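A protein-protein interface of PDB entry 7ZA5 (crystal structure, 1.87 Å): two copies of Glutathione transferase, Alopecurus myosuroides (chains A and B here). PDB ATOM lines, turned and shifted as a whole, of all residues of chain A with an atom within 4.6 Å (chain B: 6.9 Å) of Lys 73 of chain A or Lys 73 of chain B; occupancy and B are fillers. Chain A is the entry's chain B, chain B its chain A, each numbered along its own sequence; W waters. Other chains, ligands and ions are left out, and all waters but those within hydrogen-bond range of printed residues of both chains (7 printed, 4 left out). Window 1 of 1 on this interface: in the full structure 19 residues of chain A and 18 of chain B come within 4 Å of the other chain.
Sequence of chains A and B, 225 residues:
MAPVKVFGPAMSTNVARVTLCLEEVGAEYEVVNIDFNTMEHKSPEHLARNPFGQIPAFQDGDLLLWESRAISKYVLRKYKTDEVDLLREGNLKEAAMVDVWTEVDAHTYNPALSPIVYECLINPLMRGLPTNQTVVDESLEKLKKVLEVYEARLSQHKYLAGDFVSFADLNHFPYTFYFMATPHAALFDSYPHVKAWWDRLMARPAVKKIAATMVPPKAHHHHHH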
ATOM      1  N   ARG A  69      13.239 -17.371   4.596  1.00  0.00           N
ATOM      2  CA  ARG A  69      13.830 -16.038   4.660  1.00  0.00           C
ATOM      3  C   ARG A  69      14.857 -15.947   5.793  1.00  0.00           C
ATOM      4  O   ARG A  69      15.894 -15.301   5.638  1.00  0.00           O
ATOM      5  CB  ARG A  69      12.720 -14.991   4.818  1.00  0.00           C
ATOM      6  CG  ARG A  69      11.956 -14.757   3.492  1.00  0.00           C
ATOM      7  CD  ARG A  69      11.373 -13.357   3.364  1.00  0.00           C
ATOM      8  NE  ARG A  69      10.462 -13.200   2.224  1.00  0.00           N
ATOM      9  CZ  ARG A  69       9.419 -13.966   1.921  1.00  0.00           C
ATOM     10  NH1 ARG A  69       8.976 -14.905   2.749  1.00  0.00           N
ATOM     11  NH2 ARG A  69       8.772 -13.749   0.769  1.00  0.00           N
ATOM     12  N   ALA A  70      14.592 -16.597   6.932  1.00  0.00           N
ATOM     13  CA  ALA A  70      15.581 -16.627   8.013  1.00  0.00           C
ATOM     14  C   ALA A  70      16.816 -17.443   7.625  1.00  0.00           C
ATOM     15  O   ALA A  70      17.951 -17.042   7.916  1.00  0.00           O
ATOM     16  CB  ALA A  70      14.958 -17.198   9.278  1.00  0.00           C
ATOM     17  N   ILE A  71      16.616 -18.603   7.012  1.00  0.00           N
ATOM     18  CA  ILE A  71      17.745 -19.393   6.525  1.00  0.00           C
ATOM     19  C   ILE A  71      18.567 -18.598   5.525  1.00  0.00           C
ATOM     20  O   ILE A  71      19.799 -18.575   5.598  1.00  0.00           O
ATOM     21  CB  ILE A  71      17.256 -20.707   5.899  1.00  0.00           C
ATOM     22  CG1 ILE A  71      16.562 -21.571   6.950  1.00  0.00           C
ATOM     23  CG2 ILE A  71      18.426 -21.433   5.182  1.00  0.00           C
ATOM     24  CD1 ILE A  71      15.679 -22.691   6.344  1.00  0.00           C
ATOM     25  N   SER A  72      17.902 -17.956   4.560  1.00  0.00           N
ATOM     26  CA  SER A  72      18.622 -17.205   3.536  1.00  0.00           C
ATOM     27  C   SER A  72      19.484 -16.111   4.156  1.00  0.00           C
ATOM     28  O   SER A  72      20.627 -15.888   3.734  1.00  0.00           O
ATOM     29  CB  SER A  72      17.632 -16.592   2.528  1.00  0.00           C
ATOM     30  OG  SER A  72      16.925 -17.593   1.816  1.00  0.00           O
ATOM     31  N   LYS A  73      18.937 -15.389   5.140  1.00  0.00           N
ATOM     32  CA  LYS A  73      19.693 -14.288   5.726  1.00  0.00           C
ATOM     33  C   LYS A  73      20.874 -14.809   6.543  1.00  0.00           C
ATOM     34  O   LYS A  73      21.938 -14.182   6.571  1.00  0.00           O
ATOM     35  CB  LYS A  73      18.789 -13.405   6.583  1.00  0.00           C
ATOM     36  CG  LYS A  73      17.973 -12.405   5.759  1.00  0.00           C
ATOM     37  CD  LYS A  73      17.335 -11.360   6.658  1.00  0.00           C
ATOM     38  CE  LYS A  73      16.154 -11.954   7.391  1.00  0.00           C
ATOM     39  NZ  LYS A  73      15.317 -10.888   8.041  1.00  0.00           N
ATOM     40  N   TYR A  74      20.701 -15.958   7.204  1.00  0.00           N
ATOM     41  CA  TYR A  74      21.824 -16.600   7.885  1.00  0.00           C
ATOM     42  C   TYR A  74      22.934 -16.942   6.894  1.00  0.00           C
ATOM     43  O   TYR A  74      24.121 -16.690   7.156  1.00  0.00           O
ATOM     44  CB  TYR A  74      21.346 -17.851   8.619  1.00  0.00           C
ATOM     45  CG  TYR A  74      22.479 -18.681   9.203  1.00  0.00           C
ATOM     46  CD1 TYR A  74      23.036 -18.368  10.433  1.00  0.00           C
ATOM     47  CD2 TYR A  74      22.996 -19.753   8.498  1.00  0.00           C
ATOM     48  CE1 TYR A  74      24.091 -19.133  10.974  1.00  0.00           C
ATOM     49  CE2 TYR A  74      24.025 -20.514   9.012  1.00  0.00           C
ATOM     50  CZ  TYR A  74      24.567 -20.213  10.243  1.00  0.00           C
ATOM     51  OH  TYR A  74      25.584 -21.005  10.721  1.00  0.00           O
ATOM     52  N   VAL A  75      22.563 -17.462   5.721  1.00  0.00           N
ATOM     53  CA  VAL A  75      23.567 -17.834   4.724  1.00  0.00           C
ATOM     54  C   VAL A  75      24.299 -16.595   4.218  1.00  0.00           C
ATOM     55  O   VAL A  75      25.531 -16.588   4.097  1.00  0.00           O
ATOM     56  CB  VAL A  75      22.923 -18.626   3.572  1.00  0.00           C
ATOM     57  CG1 VAL A  75      23.855 -18.672   2.347  1.00  0.00           C
ATOM     58  CG2 VAL A  75      22.540 -20.052   4.042  1.00  0.00           C
ATOM     59  N   LEU A  76      23.543 -15.525   3.928  1.00  0.00           N
ATOM     60  CA  LEU A  76      24.141 -14.319   3.368  1.00  0.00           C
ATOM     61  C   LEU A  76      25.078 -13.650   4.372  1.00  0.00           C
ATOM     62  O   LEU A  76      26.055 -13.014   3.971  1.00  0.00           O
ATOM     63  CB  LEU A  76      23.046 -13.355   2.912  1.00  0.00           C
ATOM     64  CG  LEU A  76      22.145 -13.834   1.758  1.00  0.00           C
ATOM     65  CD1 LEU A  76      21.111 -12.764   1.391  1.00  0.00           C
ATOM     66  CD2 LEU A  76      22.950 -14.236   0.506  1.00  0.00           C
ATOM     67  N   ARG A  77      24.809 -13.811   5.670  1.00  0.00           N
ATOM     68  CA  ARG A  77      25.689 -13.271   6.705  1.00  0.00           C
ATOM     69  C   ARG A  77      26.905 -14.155   6.902  1.00  0.00           C
ATOM     70  O   ARG A  77      28.039 -13.662   6.976  1.00  0.00           O
ATOM     71  CB  ARG A  77      24.933 -13.132   8.035  1.00  0.00           C
ATOM     72  CG  ARG A  77      23.906 -12.012   8.064  1.00  0.00           C
ATOM     73  CD  ARG A  77      22.958 -12.146   9.263  1.00  0.00           C
ATOM     74  NE  ARG A  77      22.016 -11.034   9.309  1.00  0.00           N
ATOM     75  CZ  ARG A  77      20.772 -11.102   9.770  1.00  0.00           C
ATOM     76  NH1 ARG A  77      20.265 -12.229  10.233  1.00  0.00           N
ATOM     77  NH2 ARG A  77      20.007 -10.012   9.737  1.00  0.00           N
ATOM     78  N   LEU A  87      23.295  -8.262   1.914  1.00  0.00           N
ATOM     79  CA  LEU A  87      22.427  -7.590   2.878  1.00  0.00           C
ATOM     80  C   LEU A  87      22.876  -6.172   3.230  1.00  0.00           C
ATOM     81  O   LEU A  87      22.044  -5.388   3.697  1.00  0.00           O
ATOM     82  CB  LEU A  87      22.312  -8.405   4.179  1.00  0.00           C
ATOM     83  CG  LEU A  87      21.699  -9.808   4.056  1.00  0.00           C
ATOM     84  CD1 LEU A  87      21.883 -10.627   5.321  1.00  0.00           C
ATOM     85  CD2 LEU A  87      20.223  -9.744   3.671  1.00  0.00           C
ATOM     86  N   ASP A  99      15.843  -4.042   3.035  1.00  0.00           N
ATOM     87  CA  ASP A  99      14.731  -4.445   3.889  1.00  0.00           C
ATOM     88  C   ASP A  99      13.387  -3.985   3.319  1.00  0.00           C
ATOM     89  O   ASP A  99      12.426  -4.757   3.323  1.00  0.00           O
ATOM     90  CB  ASP A  99      14.975  -3.895   5.300  1.00  0.00           C
ATOM     91  CG  ASP A  99      16.043  -4.693   6.062  1.00  0.00           C
ATOM     92  OD1 ASP A  99      16.580  -5.690   5.486  1.00  0.00           O
ATOM     93  OD2 ASP A  99      16.455  -4.227   7.161  1.00  0.00           O
ATOM     94  N   PHE A 167      19.705  -9.192  -1.536  1.00  0.00           N
ATOM     95  CA  PHE A 167      18.631 -10.085  -1.094  1.00  0.00           C
ATOM     96  C   PHE A 167      17.268  -9.650  -1.641  1.00  0.00           C
ATOM     97  O   PHE A 167      16.396 -10.490  -1.916  1.00  0.00           O
ATOM     98  CB  PHE A 167      18.634 -10.109   0.439  1.00  0.00           C
ATOM     99  CG  PHE A 167      17.739 -11.147   1.066  1.00  0.00           C
ATOM    100  CD1 PHE A 167      17.673 -12.449   0.577  1.00  0.00           C
ATOM    101  CD2 PHE A 167      16.993 -10.824   2.201  1.00  0.00           C
ATOM    102  CE1 PHE A 167      16.854 -13.398   1.202  1.00  0.00           C
ATOM    103  CE2 PHE A 167      16.170 -11.772   2.822  1.00  0.00           C
ATOM    104  CZ  PHE A 167      16.109 -13.068   2.313  1.00  0.00           C
ATOM    105  N   CYS B  21       9.418   0.391  18.852  1.00  0.00           N
ATOM    106  CA  CYS B  21      10.851   0.209  18.658  1.00  0.00           C
ATOM    107  C   CYS B  21      11.620   1.469  19.068  1.00  0.00           C
ATOM    108  O   CYS B  21      12.672   1.381  19.715  1.00  0.00           O
ATOM    109  CB  CYS B  21      11.109  -0.140  17.195  1.00  0.00           C
ATOM    110  SG  CYS B  21      10.847  -1.941  16.871  1.00  0.00           S
ATOM    111  N   GLU B  67       7.274   0.733   5.025  1.00  0.00           N
ATOM    112  CA  GLU B  67       7.155  -0.622   5.572  1.00  0.00           C
ATOM    113  C   GLU B  67       7.671  -0.694   6.992  1.00  0.00           C
ATOM    114  O   GLU B  67       8.839  -0.399   7.267  1.00  0.00           O
ATOM    115  CB  GLU B  67       7.842  -1.707   4.718  1.00  0.00           C
ATOM    116  CG  GLU B  67       7.417  -1.770   3.249  1.00  0.00           C
ATOM    117  CD  GLU B  67       6.100  -2.487   3.047  1.00  0.00           C
ATOM    118  OE1 GLU B  67       5.693  -3.297   3.909  1.00  0.00           O
ATOM    119  OE2 GLU B  67       5.459  -2.264   2.006  1.00  0.00           O
ATOM    120  N   SER B  68       6.785  -1.095   7.899  1.00  0.00           N
ATOM    121  CA  SER B  68       7.072  -0.935   9.321  1.00  0.00           C
ATOM    122  C   SER B  68       8.224  -1.826   9.767  1.00  0.00           C
ATOM    123  O   SER B  68       9.012  -1.422  10.619  1.00  0.00           O
ATOM    124  CB  SER B  68       5.810  -1.224  10.141  1.00  0.00           C
ATOM    125  OG  SER B  68       5.366  -2.551   9.937  1.00  0.00           O
ATOM    126  N   ARG B  69       8.342  -3.044   9.214  1.00  0.00           N
ATOM    127  CA  ARG B  69       9.446  -3.908   9.635  1.00  0.00           C
ATOM    128  C   ARG B  69      10.796  -3.400   9.134  1.00  0.00           C
ATOM    129  O   ARG B  69      11.798  -3.521   9.843  1.00  0.00           O
ATOM    130  CB  ARG B  69       9.215  -5.356   9.181  1.00  0.00           C
ATOM    131  CG  ARG B  69       8.159  -6.088  10.020  1.00  0.00           C
ATOM    132  CD  ARG B  69       7.825  -7.475   9.474  1.00  0.00           C
ATOM    133  NE  ARG B  69       6.700  -8.069  10.181  1.00  0.00           N
ATOM    134  CZ  ARG B  69       5.436  -7.873   9.841  1.00  0.00           C
ATOM    135  NH1 ARG B  69       5.118  -7.129   8.796  1.00  0.00           N
ATOM    136  NH2 ARG B  69       4.476  -8.484  10.526  1.00  0.00           N
ATOM    137  N   ALA B  70      10.850  -2.806   7.939  1.00  0.00           N
ATOM    138  CA  ALA B  70      12.108  -2.208   7.494  1.00  0.00           C
ATOM    139  C   ALA B  70      12.468  -0.987   8.341  1.00  0.00           C
ATOM    140  O   ALA B  70      13.627  -0.820   8.775  1.00  0.00           O
ATOM    141  CB  ALA B  70      11.998  -1.837   6.006  1.00  0.00           C
ATOM    142  N   ILE B  71      11.489  -0.115   8.599  1.00  0.00           N
ATOM    143  CA  ILE B  71      11.743   1.026   9.476  1.00  0.00           C
ATOM    144  C   ILE B  71      12.181   0.544  10.854  1.00  0.00           C
ATOM    145  O   ILE B  71      13.154   1.042  11.429  1.00  0.00           O
ATOM    146  CB  ILE B  71      10.497   1.921   9.583  1.00  0.00           C
ATOM    147  CG1 ILE B  71      10.099   2.473   8.220  1.00  0.00           C
ATOM    148  CG2 ILE B  71      10.749   3.035  10.594  1.00  0.00           C
ATOM    149  CD1 ILE B  71       8.655   2.947   8.179  1.00  0.00           C
ATOM    150  N   SER B  72      11.444  -0.410  11.421  1.00  0.00           N
ATOM    151  CA  SER B  72      11.767  -0.885  12.768  1.00  0.00           C
ATOM    152  C   SER B  72      13.207  -1.381  12.853  1.00  0.00           C
ATOM    153  O   SER B  72      13.916  -1.104  13.830  1.00  0.00           O
ATOM    154  CB  SER B  72      10.796  -1.987  13.170  1.00  0.00           C
ATOM    155  OG  SER B  72       9.488  -1.459  13.321  1.00  0.00           O
ATOM    156  N   LYS B  73      13.666  -2.115  11.836  1.00  0.00           N
ATOM    157  CA  LYS B  73      15.018  -2.656  11.902  1.00  0.00           C
ATOM    158  C   LYS B  73      16.067  -1.545  11.770  1.00  0.00           C
ATOM    159  O   LYS B  73      17.097  -1.572  12.452  1.00  0.00           O
ATOM    160  CB  LYS B  73      15.190  -3.721  10.823  1.00  0.00           C
ATOM    161  CG  LYS B  73      14.696  -5.088  11.296  1.00  0.00           C
ATOM    162  CD  LYS B  73      15.084  -6.216  10.353  1.00  0.00           C
ATOM    163  CE  LYS B  73      14.306  -6.149   9.064  1.00  0.00           C
ATOM    164  NZ  LYS B  73      14.451  -7.416   8.267  1.00  0.00           N
ATOM    165  N   TYR B  74      15.825  -0.561  10.899  1.00  0.00           N
ATOM    166  CA  TYR B  74      16.697   0.608  10.829  1.00  0.00           C
ATOM    167  C   TYR B  74      16.837   1.279  12.204  1.00  0.00           C
ATOM    168  O   TYR B  74      17.942   1.655  12.629  1.00  0.00           O
ATOM    169  CB  TYR B  74      16.154   1.602   9.787  1.00  0.00           C
ATOM    170  CG  TYR B  74      16.933   2.912   9.772  1.00  0.00           C
ATOM    171  CD1 TYR B  74      18.128   3.025   9.067  1.00  0.00           C
ATOM    172  CD2 TYR B  74      16.474   4.016  10.483  1.00  0.00           C
ATOM    173  CE1 TYR B  74      18.856   4.238   9.066  1.00  0.00           C
ATOM    174  CE2 TYR B  74      17.183   5.217  10.485  1.00  0.00           C
ATOM    175  CZ  TYR B  74      18.372   5.319   9.776  1.00  0.00           C
ATOM    176  OH  TYR B  74      19.066   6.508   9.797  1.00  0.00           O
ATOM    177  N   VAL B  75      15.724   1.408  12.924  1.00  0.00           N
ATOM    178  CA  VAL B  75      15.752   2.038  14.242  1.00  0.00           C
ATOM    179  C   VAL B  75      16.572   1.192  15.217  1.00  0.00           C
ATOM    180  O   VAL B  75      17.438   1.702  15.944  1.00  0.00           O
ATOM    181  CB  VAL B  75      14.320   2.264  14.759  1.00  0.00           C
ATOM    182  CG1 VAL B  75      14.328   2.522  16.277  1.00  0.00           C
ATOM    183  CG2 VAL B  75      13.638   3.421  14.003  1.00  0.00           C
ATOM    184  N   LEU B  76      16.334  -0.125  15.216  1.00  0.00           N
ATOM    185  CA  LEU B  76      17.001  -0.999  16.175  1.00  0.00           C
ATOM    186  C   LEU B  76      18.499  -1.117  15.894  1.00  0.00           C
ATOM    187  O   LEU B  76      19.284  -1.384  16.816  1.00  0.00           O
ATOM    188  CB  LEU B  76      16.314  -2.372  16.173  1.00  0.00           C
ATOM    189  CG  LEU B  76      14.859  -2.443  16.648  1.00  0.00           C
ATOM    190  CD1 LEU B  76      14.387  -3.912  16.657  1.00  0.00           C
ATOM    191  CD2 LEU B  76      14.690  -1.846  18.042  1.00  0.00           C
ATOM    192  N   ARG B  77      18.924  -0.902  14.647  1.00  0.00           N
ATOM    193  CA  ARG B  77      20.349  -0.900  14.337  1.00  0.00           C
ATOM    194  C   ARG B  77      20.995   0.439  14.678  1.00  0.00           C
ATOM    195  O   ARG B  77      22.067   0.476  15.286  1.00  0.00           O
ATOM    196  CB  ARG B  77      20.573  -1.205  12.854  1.00  0.00           C
ATOM    197  CG  ARG B  77      20.403  -2.663  12.507  1.00  0.00           C
ATOM    198  CD  ARG B  77      20.314  -2.858  11.020  1.00  0.00           C
ATOM    199  NE  ARG B  77      19.969  -4.240  10.699  1.00  0.00           N
ATOM    200  CZ  ARG B  77      19.272  -4.599   9.631  1.00  0.00           C
ATOM    201  NH1 ARG B  77      18.808  -3.695   8.772  1.00  0.00           N
ATOM    202  NH2 ARG B  77      19.043  -5.892   9.415  1.00  0.00           N
ATOM    203  N   LYS B  78      20.360   1.539  14.271  1.00  0.00           N
ATOM    204  CA  LYS B  78      20.951   2.863  14.462  1.00  0.00           C
ATOM    205  C   LYS B  78      21.176   3.171  15.939  1.00  0.00           C
ATOM    206  O   LYS B  78      22.233   3.681  16.318  1.00  0.00           O
ATOM    207  CB  LYS B  78      20.068   3.940  13.835  1.00  0.00           C
ATOM    208  CG  LYS B  78      20.538   5.389  14.187  1.00  0.00           C
ATOM    209  CD  LYS B  78      19.712   6.438  13.474  1.00  0.00           C
ATOM    210  CE  LYS B  78      20.158   7.858  13.824  1.00  0.00           C
ATOM    211  NZ  LYS B  78      19.040   8.798  13.565  1.00  0.00           N
ATOM    212  N   LEU B  87      18.168  -6.981  17.818  1.00  0.00           N
ATOM    213  CA  LEU B  87      18.336  -7.809  16.625  1.00  0.00           C
ATOM    214  C   LEU B  87      19.391  -8.898  16.783  1.00  0.00           C
ATOM    215  O   LEU B  87      19.321  -9.910  16.074  1.00  0.00           O
ATOM    216  CB  LEU B  87      18.695  -6.942  15.414  1.00  0.00           C
ATOM    217  CG  LEU B  87      17.582  -5.987  14.979  1.00  0.00           C
ATOM    218  CD1 LEU B  87      18.013  -5.149  13.786  1.00  0.00           C
ATOM    219  CD2 LEU B  87      16.319  -6.766  14.661  1.00  0.00           C
ATOM    220  N   GLU B  89      22.585  -9.025  16.041  1.00  0.00           N
ATOM    221  CA  GLU B  89      23.268  -9.251  14.772  1.00  0.00           C
ATOM    222  C   GLU B  89      24.744  -9.614  14.921  1.00  0.00           C
ATOM    223  O   GLU B  89      25.321 -10.156  13.970  1.00  0.00           O
ATOM    224  CB  GLU B  89      23.091  -8.025  13.857  1.00  0.00           C
ATOM    225  CG  GLU B  89      21.693  -7.997  13.228  1.00  0.00           C
ATOM    226  CD  GLU B  89      21.394  -6.750  12.383  1.00  0.00           C
ATOM    227  OE1 GLU B  89      22.133  -5.749  12.440  1.00  0.00           O
ATOM    228  OE2 GLU B  89      20.401  -6.795  11.637  1.00  0.00           O
ATOM    229  N   LEU B  92      25.348 -14.727  14.986  1.00  0.00           N
ATOM    230  CA  LEU B  92      24.549 -15.169  13.841  1.00  0.00           C
ATOM    231  C   LEU B  92      23.475 -16.163  14.246  1.00  0.00           C
ATOM    232  O   LEU B  92      22.387 -16.172  13.669  1.00  0.00           O
ATOM    233  CB  LEU B  92      25.439 -15.786  12.759  1.00  0.00           C
ATOM    234  CG  LEU B  92      26.466 -14.839  12.129  1.00  0.00           C
ATOM    235  CD1 LEU B  92      26.921 -15.380  10.782  1.00  0.00           C
ATOM    236  CD2 LEU B  92      25.863 -13.457  11.977  1.00  0.00           C
ATOM    237  N   ALA B  95      20.673 -14.143  15.988  1.00  0.00           N
ATOM    238  CA  ALA B  95      19.964 -13.372  14.965  1.00  0.00           C
ATOM    239  C   ALA B  95      19.098 -14.281  14.092  1.00  0.00           C
ATOM    240  O   ALA B  95      17.998 -13.897  13.664  1.00  0.00           O
ATOM    241  CB  ALA B  95      20.970 -12.593  14.120  1.00  0.00           C
ATOM    242  N   ASP B  99      15.079 -13.900  13.474  1.00  0.00           N
ATOM    243  CA  ASP B  99      14.495 -13.891  12.139  1.00  0.00           C
ATOM    244  C   ASP B  99      13.429 -14.978  11.987  1.00  0.00           C
ATOM    245  O   ASP B  99      12.375 -14.747  11.386  1.00  0.00           O
ATOM    246  CB  ASP B  99      15.600 -14.045  11.089  1.00  0.00           C
ATOM    247  CG  ASP B  99      16.474 -12.788  10.969  1.00  0.00           C
ATOM    248  OD1 ASP B  99      16.120 -11.729  11.550  1.00  0.00           O
ATOM    249  OD2 ASP B  99      17.545 -12.856  10.319  1.00  0.00           O
ATOM    250  N   THR B 102      10.316 -13.787  13.774  1.00  0.00           N
ATOM    251  CA  THR B 102       9.743 -12.662  13.050  1.00  0.00           C
ATOM    252  C   THR B 102       8.948 -13.162  11.846  1.00  0.00           C
ATOM    253  O   THR B 102       7.855 -12.662  11.557  1.00  0.00           O
ATOM    254  CB  THR B 102      10.850 -11.698  12.628  1.00  0.00           C
ATOM    255  OG1 THR B 102      11.449 -11.115  13.799  1.00  0.00           O
ATOM    256  CG2 THR B 102      10.290 -10.581  11.745  1.00  0.00           C
ATOM    257  N   GLU B 103       9.472 -14.168  11.138  1.00  0.00           N
ATOM    258  CA  GLU B 103       8.732 -14.686   9.993  1.00  0.00           C
ATOM    259  C   GLU B 103       7.500 -15.475  10.426  1.00  0.00           C
ATOM    260  O   GLU B 103       6.462 -15.434   9.750  1.00  0.00           O
ATOM    261  CB  GLU B 103       9.607 -15.566   9.112  1.00  0.00           C
ATOM    262  CG  GLU B 103      10.791 -14.859   8.513  1.00  0.00           C
ATOM    263  CD  GLU B 103      10.366 -13.791   7.529  1.00  0.00           C
ATOM    264  OE1 GLU B 103       9.703 -14.118   6.535  1.00  0.00           O
ATOM    265  OE2 GLU B 103      10.796 -12.620   7.727  1.00  0.00           O
ATOM    266  N   PHE B 167      13.396  -8.290  18.885  1.00  0.00           N
ATOM    267  CA  PHE B 167      12.462  -7.834  17.863  1.00  0.00           C
ATOM    268  C   PHE B 167      11.379  -8.876  17.598  1.00  0.00           C
ATOM    269  O   PHE B 167      10.233  -8.521  17.307  1.00  0.00           O
ATOM    270  CB  PHE B 167      13.260  -7.522  16.590  1.00  0.00           C
ATOM    271  CG  PHE B 167      12.456  -6.927  15.455  1.00  0.00           C
ATOM    272  CD1 PHE B 167      11.561  -5.895  15.665  1.00  0.00           C
ATOM    273  CD2 PHE B 167      12.643  -7.397  14.152  1.00  0.00           C
ATOM    274  CE1 PHE B 167      10.863  -5.339  14.597  1.00  0.00           C
ATOM    275  CE2 PHE B 167      11.954  -6.843  13.089  1.00  0.00           C
ATOM    276  CZ  PHE B 167      11.058  -5.812  13.317  1.00  0.00           C
HETATM  277  O   HOH W   1      13.092 -12.229   9.291  1.00  0.00           O
HETATM  278  O   HOH W   2      21.516 -14.900  10.978  1.00  0.00           O
HETATM  279  O   HOH W   3      16.141  -1.652   7.739  1.00  0.00           O
HETATM  280  O   HOH W   4      12.886  -6.938   5.723  1.00  0.00           O
HETATM  281  O   HOH W   5      13.302  -9.385   9.636  1.00  0.00           O
HETATM  282  O   HOH W   6      14.445  -9.211   5.909  1.00  0.00           O
HETATM  283  O   HOH W   7      18.895 -15.330   9.953  1.00  0.00           O
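The side-chain carboxylate (OE1) of Glu 103 of chain B is in salt-bridge range of the guanidinium group (NH1) of Arg 69 of chain A (3.9 Å). The guanidinium group (NH1) of Arg 77 of chain A is in salt-bridge range of the side-chain carboxylate (OD2) of Asp 99 of chain B, 2.8 Å away. The side-chain carboxylate (OD1) of Asp 99 of chain B lies within salt-bridge range of the side-chain amino group (NZ) of Lys 73 of chain A, 3.7 Å away. The side-chain amino group of Lys 73 of chain B is in salt-bridge range of the side-chain carboxylate of Asp 99 of chain A (3.9 Å). OD2 of Asp 99 of chain A is in salt-bridge range of NH1 of Arg 77 of chain B (2.9 Å). The guanidinium group of Arg 77 of chain A lies within salt-bridge range of the side-chain carboxylate of Glu 89 of chain B (3.8 Å).
The guanidinium group (NE) of Arg 77 of chain B is in salt-bridge range of the side-chain carboxylate (OE2) of Glu 89 of chain B, at 2.8 Å.
Ala 70 of chain A touches Asp 99 of chain B. Lys 73 of chain B touches Lys 73 of chain A (NZ to NZ, 3.6 Å). Leu 92 of chain B touches Tyr 74 of chain A (O to CD1, 3.96 Å). Ala 95 of chain B touches Arg 77 of chain A (CB to NH1, 3.97 Å). Asp 99 of chain A touches Ala 70 of chain B (CB to CB, 3.7 Å).
Lys 73 of chain A touches just these residues of chain B: Lys 73 and Asp 99. Lys 73 of chain B touches two residues of chain A. Of the printed residues of chain A, Arg 77 of chain B touches Asp 99. Printed residues of chain A within 4 Å of Ala 70 of chain B: Asp 99 (3.7 Å). Of the printed residues of chain B, Tyr 74 of chain A touches Leu 92. Of the printed residues of chain B, Arg 69 of chain A touches Glu 103. Of the printed residues of chain B, Arg 77 of chain A touches Glu 89 (3.8 Å), Ala 95 (3.97 Å) and Asp 99 (2.8 Å). Arg 69 of chain B touches none of the printed residues of chain A. The nearest residue of chain B that does not touch Lys 73 of chain A is Glu 103 of chain B (4.9 Å).
Printed residues of chain A that touch a printed residue of chain B: Arg 69, Ala 70, Lys 73, Tyr 74, Arg 77 and Asp 99. Along chain A the printed residues that touch a printed residue of chain B span positions 69 to 99. Of the 21 printed residues of chain B, 8 touch a printed residue of chain A. Printed residues of chain B that touch a printed residue of chain A: Ala 70, Lys 73, Arg 77, Glu 89, Leu 92, Ala 95, Asp 99 and Glu 103. Hydrophobic or aromatic side chains of chain B within 4 Å of the printed part of chain A: Ala 70 and Ala 95.
Ala 70 of chain A touches Asp 99 of chain B, and with the chains exchanged Asp 99 of chain A touches Ala 70 of chain B. Lys 73 of chain B touches its own counterpart, Lys 73 of chain A. Lys 73 of chain A touches Asp 99 of chain B, and with the chains exchanged Asp 99 of chain A touches Lys 73 of chain B. Arg 77 of chain A touches Asp 99 of chain B, and with the chains exchanged Asp 99 of chain A touches Arg 77 of chain B. Of the 11 pairs that touch across the chains among the printed residues, 7 have their exchanged pair printed and touching as well.
Water W3 lies within hydrogen-bond range of the side-chain carboxylate of Asp 99 of chain A, the backbone carbonyl oxygen of Ala 70 of chain B and the backbone NH of Tyr 74 of chain B. Water W5 bridges NZ of Lys 73 of chain B and NZ of Lys 73 of chain A. Water W1 lies within hydrogen-bond range of OE2 of Glu 103 of chain B, NZ of Lys 73 of chain A and O of Asp 99 of chain B. Water W7 lies within hydrogen-bond range of the backbone carbonyl oxygen of Ala 70 of chain A (2.8 Å), the side-chain carboxylate of Asp 99 of chain B (2.8 Å), the backbone NH of Tyr 74 of chain A (3.3 Å) and the guanidinium group of Arg 77 of chain A (3.4 Å). Water W4 lies within hydrogen-bond range of the side-chain amino group (NZ) of Lys 73 of chain B (3.0 Å) and the backbone carbonyl oxygen (O) of Asp 99 of chain A (3.3 Å). Water W2 lies within hydrogen-bond range of NH1 of Arg 77 of chain A and O of Leu 92 of chain B.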
